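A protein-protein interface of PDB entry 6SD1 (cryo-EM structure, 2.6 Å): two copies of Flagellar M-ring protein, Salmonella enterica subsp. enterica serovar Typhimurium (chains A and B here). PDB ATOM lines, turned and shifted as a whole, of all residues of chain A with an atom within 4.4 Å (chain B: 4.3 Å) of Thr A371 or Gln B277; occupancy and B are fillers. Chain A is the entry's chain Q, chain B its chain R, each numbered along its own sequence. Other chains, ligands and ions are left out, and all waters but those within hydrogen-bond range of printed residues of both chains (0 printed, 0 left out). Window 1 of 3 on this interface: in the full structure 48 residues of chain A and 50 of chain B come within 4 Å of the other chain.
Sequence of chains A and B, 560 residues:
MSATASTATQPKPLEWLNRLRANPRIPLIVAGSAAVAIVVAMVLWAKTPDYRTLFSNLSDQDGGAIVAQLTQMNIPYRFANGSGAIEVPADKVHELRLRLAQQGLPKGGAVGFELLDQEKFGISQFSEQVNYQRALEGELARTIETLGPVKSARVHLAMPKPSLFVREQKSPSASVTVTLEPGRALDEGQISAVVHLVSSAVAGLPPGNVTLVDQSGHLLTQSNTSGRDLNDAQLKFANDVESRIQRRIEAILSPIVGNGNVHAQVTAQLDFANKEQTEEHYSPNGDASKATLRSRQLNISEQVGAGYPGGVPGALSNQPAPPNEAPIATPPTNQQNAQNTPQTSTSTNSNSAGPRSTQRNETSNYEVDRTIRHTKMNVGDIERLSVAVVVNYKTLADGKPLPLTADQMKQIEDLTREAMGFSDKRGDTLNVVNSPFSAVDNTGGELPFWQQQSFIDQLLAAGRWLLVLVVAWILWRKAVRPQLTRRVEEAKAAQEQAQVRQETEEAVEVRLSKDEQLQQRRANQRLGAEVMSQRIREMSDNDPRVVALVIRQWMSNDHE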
ATOM      1  N   GLU A 279       2.124 -22.356   6.728  1.00  0.00           N
ATOM      2  CA  GLU A 279       2.379 -21.543   5.554  1.00  0.00           C
ATOM      3  C   GLU A 279       3.726 -21.919   4.949  1.00  0.00           C
ATOM      4  O   GLU A 279       4.547 -22.598   5.568  1.00  0.00           O
ATOM      5  CB  GLU A 279       2.357 -20.059   5.905  1.00  0.00           C
ATOM      6  CG  GLU A 279       1.193 -19.647   6.777  1.00  0.00           C
ATOM      7  CD  GLU A 279       1.377 -18.264   7.371  1.00  0.00           C
ATOM      8  OE1 GLU A 279       2.309 -17.551   6.943  1.00  0.00           O
ATOM      9  OE2 GLU A 279       0.596 -17.891   8.272  1.00  0.00           O
ATOM     10  N   GLU A 280       3.945 -21.475   3.716  1.00  0.00           N
ATOM     11  CA  GLU A 280       5.192 -21.770   3.016  1.00  0.00           C
ATOM     12  C   GLU A 280       5.348 -20.739   1.905  1.00  0.00           C
ATOM     13  O   GLU A 280       5.040 -21.025   0.748  1.00  0.00           O
ATOM     14  CB  GLU A 280       5.196 -23.188   2.467  1.00  0.00           C
ATOM     15  CG  GLU A 280       6.571 -23.705   2.115  1.00  0.00           C
ATOM     16  CD  GLU A 280       6.566 -25.176   1.754  1.00  0.00           C
ATOM     17  OE1 GLU A 280       5.467 -25.753   1.620  1.00  0.00           O
ATOM     18  OE2 GLU A 280       7.663 -25.754   1.601  1.00  0.00           O
ATOM     19  N   HIS A 281       5.831 -19.557   2.263  1.00  0.00           N
ATOM     20  CA  HIS A 281       5.992 -18.458   1.327  1.00  0.00           C
ATOM     21  C   HIS A 281       7.347 -18.535   0.636  1.00  0.00           C
ATOM     22  O   HIS A 281       8.344 -18.954   1.225  1.00  0.00           O
ATOM     23  CB  HIS A 281       5.846 -17.115   2.045  1.00  0.00           C
ATOM     24  CG  HIS A 281       6.011 -15.927   1.148  1.00  0.00           C
ATOM     25  ND1 HIS A 281       4.953 -15.337   0.492  1.00  0.00           N
ATOM     26  CD2 HIS A 281       7.112 -15.219   0.800  1.00  0.00           C
ATOM     27  CE1 HIS A 281       5.394 -14.317  -0.223  1.00  0.00           C
ATOM     28  NE2 HIS A 281       6.701 -14.225  -0.054  1.00  0.00           N
ATOM     29  N   ARG A 370      12.833 -19.065   1.123  1.00  0.00           N
ATOM     30  CA  ARG A 370      11.666 -19.816   1.573  1.00  0.00           C
ATOM     31  C   ARG A 370      11.478 -19.639   3.070  1.00  0.00           C
ATOM     32  O   ARG A 370      12.413 -19.860   3.843  1.00  0.00           O
ATOM     33  CB  ARG A 370      11.815 -21.295   1.225  1.00  0.00           C
ATOM     34  CG  ARG A 370      10.619 -22.132   1.601  1.00  0.00           C
ATOM     35  CD  ARG A 370      10.824 -23.571   1.201  1.00  0.00           C
ATOM     36  NE  ARG A 370      11.917 -24.183   1.939  1.00  0.00           N
ATOM     37  CZ  ARG A 370      11.963 -25.469   2.267  1.00  0.00           C
ATOM     38  NH1 ARG A 370      10.974 -26.278   1.916  1.00  0.00           N
ATOM     39  NH2 ARG A 370      12.999 -25.945   2.942  1.00  0.00           N
ATOM     40  N   THR A 371      10.271 -19.253   3.468  1.00  0.00           N
ATOM     41  CA  THR A 371       9.869 -19.205   4.866  1.00  0.00           C
ATOM     42  C   THR A 371       8.771 -20.229   5.109  1.00  0.00           C
ATOM     43  O   THR A 371       7.845 -20.358   4.308  1.00  0.00           O
ATOM     44  CB  THR A 371       9.364 -17.814   5.250  1.00  0.00           C
ATOM     45  OG1 THR A 371      10.243 -16.818   4.716  1.00  0.00           O
ATOM     46  CG2 THR A 371       9.303 -17.672   6.755  1.00  0.00           C
ATOM     47  N   ILE A 372       8.877 -20.956   6.217  1.00  0.00           N
ATOM     48  CA  ILE A 372       7.904 -21.977   6.581  1.00  0.00           C
ATOM     49  C   ILE A 372       7.470 -21.722   8.017  1.00  0.00           C
ATOM     50  O   ILE A 372       8.195 -22.062   8.958  1.00  0.00           O
ATOM     51  CB  ILE A 372       8.464 -23.396   6.427  1.00  0.00           C
ATOM     52  CG1 ILE A 372       8.873 -23.647   4.977  1.00  0.00           C
ATOM     53  CG2 ILE A 372       7.433 -24.421   6.858  1.00  0.00           C
ATOM     54  CD1 ILE A 372       9.542 -24.981   4.753  1.00  0.00           C
ATOM     55  N   ARG A 373       6.290 -21.133   8.186  1.00  0.00           N
ATOM     56  CA  ARG A 373       5.690 -20.926   9.496  1.00  0.00           C
ATOM     57  C   ARG A 373       4.732 -22.068   9.795  1.00  0.00           C
ATOM     58  O   ARG A 373       3.912 -22.430   8.950  1.00  0.00           O
ATOM     59  CB  ARG A 373       4.945 -19.594   9.555  1.00  0.00           C
ATOM     60  CG  ARG A 373       5.814 -18.382   9.326  1.00  0.00           C
ATOM     61  CD  ARG A 373       4.978 -17.125   9.159  1.00  0.00           C
ATOM     62  NE  ARG A 373       4.051 -16.911  10.265  1.00  0.00           N
ATOM     63  CZ  ARG A 373       4.369 -16.314  11.409  1.00  0.00           C
ATOM     64  NH1 ARG A 373       5.601 -15.868  11.609  1.00  0.00           N
ATOM     65  NH2 ARG A 373       3.454 -16.158  12.353  1.00  0.00           N
ATOM     66  N   GLU B 276       6.308 -22.230  15.011  1.00  0.00           N
ATOM     67  CA  GLU B 276       7.612 -22.526  14.444  1.00  0.00           C
ATOM     68  C   GLU B 276       7.836 -21.633  13.234  1.00  0.00           C
ATOM     69  O   GLU B 276       6.891 -21.138  12.620  1.00  0.00           O
ATOM     70  CB  GLU B 276       7.713 -23.993  14.017  1.00  0.00           C
ATOM     71  CG  GLU B 276       7.499 -25.008  15.120  1.00  0.00           C
ATOM     72  CD  GLU B 276       8.599 -25.007  16.147  1.00  0.00           C
ATOM     73  OE1 GLU B 276       9.748 -24.676  15.788  1.00  0.00           O
ATOM     74  OE2 GLU B 276       8.317 -25.356  17.314  1.00  0.00           O
ATOM     75  N   GLN B 277       9.101 -21.428  12.891  1.00  0.00           N
ATOM     76  CA  GLN B 277       9.427 -20.688  11.685  1.00  0.00           C
ATOM     77  C   GLN B 277      10.826 -21.066  11.235  1.00  0.00           C
ATOM     78  O   GLN B 277      11.720 -21.262  12.061  1.00  0.00           O
ATOM     79  CB  GLN B 277       9.329 -19.177  11.897  1.00  0.00           C
ATOM     80  CG  GLN B 277       9.333 -18.391  10.605  1.00  0.00           C
ATOM     81  CD  GLN B 277       9.322 -16.902  10.831  1.00  0.00           C
ATOM     82  OE1 GLN B 277       9.418 -16.435  11.963  1.00  0.00           O
ATOM     83  NE2 GLN B 277       9.202 -16.142   9.753  1.00  0.00           N
ATOM     84  N   THR B 278      11.002 -21.173   9.922  1.00  0.00           N
ATOM     85  CA  THR B 278      12.291 -21.486   9.315  1.00  0.00           C
ATOM     86  C   THR B 278      12.437 -20.618   8.071  1.00  0.00           C
ATOM     87  O   THR B 278      11.870 -20.927   7.022  1.00  0.00           O
ATOM     88  CB  THR B 278      12.404 -22.966   8.968  1.00  0.00           C
ATOM     89  OG1 THR B 278      12.120 -23.753  10.130  1.00  0.00           O
ATOM     90  CG2 THR B 278      13.803 -23.290   8.490  1.00  0.00           C
ATOM     91  N   GLU B 279      13.184 -19.528   8.195  1.00  0.00           N
ATOM     92  CA  GLU B 279      13.542 -18.739   7.032  1.00  0.00           C
ATOM     93  C   GLU B 279      14.725 -19.381   6.317  1.00  0.00           C
ATOM     94  O   GLU B 279      15.379 -20.289   6.834  1.00  0.00           O
ATOM     95  CB  GLU B 279      13.888 -17.307   7.432  1.00  0.00           C
ATOM     96  CG  GLU B 279      12.750 -16.532   8.068  1.00  0.00           C
ATOM     97  CD  GLU B 279      12.842 -16.483   9.587  1.00  0.00           C
ATOM     98  OE1 GLU B 279      13.364 -17.442  10.194  1.00  0.00           O
ATOM     99  OE2 GLU B 279      12.406 -15.471  10.174  1.00  0.00           O
ATOM    100  N   ARG B 373      17.677 -19.165   9.287  1.00  0.00           N
ATOM    101  CA  ARG B 373      17.199 -18.888  10.634  1.00  0.00           C
ATOM    102  C   ARG B 373      16.083 -19.860  10.981  1.00  0.00           C
ATOM    103  O   ARG B 373      15.204 -20.122  10.157  1.00  0.00           O
ATOM    104  CB  ARG B 373      16.694 -17.451  10.751  1.00  0.00           C
ATOM    105  CG  ARG B 373      17.745 -16.399  10.484  1.00  0.00           C
ATOM    106  CD  ARG B 373      17.129 -15.019  10.342  1.00  0.00           C
ATOM    107  NE  ARG B 373      16.358 -14.619  11.516  1.00  0.00           N
ATOM    108  CZ  ARG B 373      16.879 -14.074  12.610  1.00  0.00           C
ATOM    109  NH1 ARG B 373      18.185 -13.865  12.697  1.00  0.00           N
ATOM    110  NH2 ARG B 373      16.092 -13.738  13.622  1.00  0.00           N
ATOM    111  N   HIS B 374      16.124 -20.401  12.192  1.00  0.00           N
ATOM    112  CA  HIS B 374      15.073 -21.271  12.701  1.00  0.00           C
ATOM    113  C   HIS B 374      14.649 -20.746  14.064  1.00  0.00           C
ATOM    114  O   HIS B 374      15.425 -20.801  15.023  1.00  0.00           O
ATOM    115  CB  HIS B 374      15.541 -22.721  12.788  1.00  0.00           C
ATOM    116  CG  HIS B 374      14.532 -23.638  13.405  1.00  0.00           C
ATOM    117  ND1 HIS B 374      13.178 -23.492  13.203  1.00  0.00           N
ATOM    118  CD2 HIS B 374      14.679 -24.705  14.223  1.00  0.00           C
ATOM    119  CE1 HIS B 374      12.532 -24.431  13.871  1.00  0.00           C
ATOM    120  NE2 HIS B 374      13.420 -25.181  14.497  1.00  0.00           N
ATOM    121  N   THR B 375      13.426 -20.237  14.150  1.00  0.00           N
ATOM    122  CA  THR B 375      12.911 -19.625  15.365  1.00  0.00           C
ATOM    123  C   THR B 375      11.751 -20.439  15.912  1.00  0.00           C
ATOM    124  O   THR B 375      10.771 -20.688  15.205  1.00  0.00           O
ATOM    125  CB  THR B 375      12.454 -18.188  15.110  1.00  0.00           C
ATOM    126  OG1 THR B 375      13.447 -17.497  14.345  1.00  0.00           O
ATOM    127  CG2 THR B 375      12.236 -17.468  16.423  1.00  0.00           C
ATOM    128  N   MET B 377       9.123 -19.742  18.501  1.00  0.00           N
ATOM    129  CA  MET B 377       8.623 -18.584  19.224  1.00  0.00           C
ATOM    130  C   MET B 377       8.224 -18.955  20.647  1.00  0.00           C
ATOM    131  O   MET B 377       7.975 -20.118  20.974  1.00  0.00           O
ATOM    132  CB  MET B 377       7.435 -17.963  18.493  1.00  0.00           C
ATOM    133  CG  MET B 377       7.709 -17.645  17.038  1.00  0.00           C
ATOM    134  SD  MET B 377       8.380 -15.992  16.808  1.00  0.00           S
ATOM    135  CE  MET B 377       8.525 -15.932  15.025  1.00  0.00           C
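The backbone carbonyl oxygen (O) of Ile A372 is in hydrogen-bond range of the backbone NH (N) of Thr B278. The backbone carbonyl oxygen (O) of Arg A370 lies close to the backbone carbonyl oxygen (O) of Thr B278, 3.4 Å away.
The side-chain carboxylate of Glu A279 lies within salt-bridge range of the guanidinium group of Arg A373 (3.8 Å). The side-chain carboxylate of Glu A280 lies within salt-bridge range of the guanidinium group of Arg A370 (3.4 Å). O of His A281 is in hydrogen-bond range of N of Thr A371, at 3.0 Å. NE2 of Gln B277 is in hydrogen-bond range of OE2 of Glu B279 (3.3 Å). ND1 of His B374 sits at hydrogen-bond distance from OG1 of Thr B278 (3.3 Å). N of Glu B279 sits at hydrogen-bond distance from O of Arg B373 (2.9 Å).
Arg A370 touches Glu B279 (O to C, 3.4 Å). CG2 of Thr A371 touches NE2 of Gln B277, 3.4 Å away. Thr B278 touches Thr A371 (O to CA, 3.4 Å). Thr A371 touches Glu B279 (CG2 to CG, 3.9 Å). Ile A372 touches Glu B276 (O to O, 3.996 Å). O of Ile A372 touches CA of Gln B277, at 3.3 Å. Arg A373 touches Glu B276. Gln B277 touches Arg A373 (CG to CG, 3.7 Å).
Thr A371 touches just these residues of chain B: Gln B277, Thr B278 and Glu B279. Gln B277 touches just these residues of chain A: Thr A371 (3.4 Å), Ile A372 (3.3 Å) and Arg A373 (3.7 Å). Printed residues of chain B within 4 Å of Arg A373: Glu B276 and Gln B277. Of the printed residues of chain A, Glu B279 touches Arg A370 and Thr A371. The nearest printed residue of chain A that does not touch Gln B277 is Arg A370 (7.6 Å).
Printed residues of chain B that touch a printed residue of chain A: Glu B276, Gln B277, Thr B278 and Glu B279. Among the printed residues, no Asp or Glu carboxylate lies within 4 Å of a Lys or Arg side-chain nitrogen of the other chain.
Positions printed for both chains: 279 and 373.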
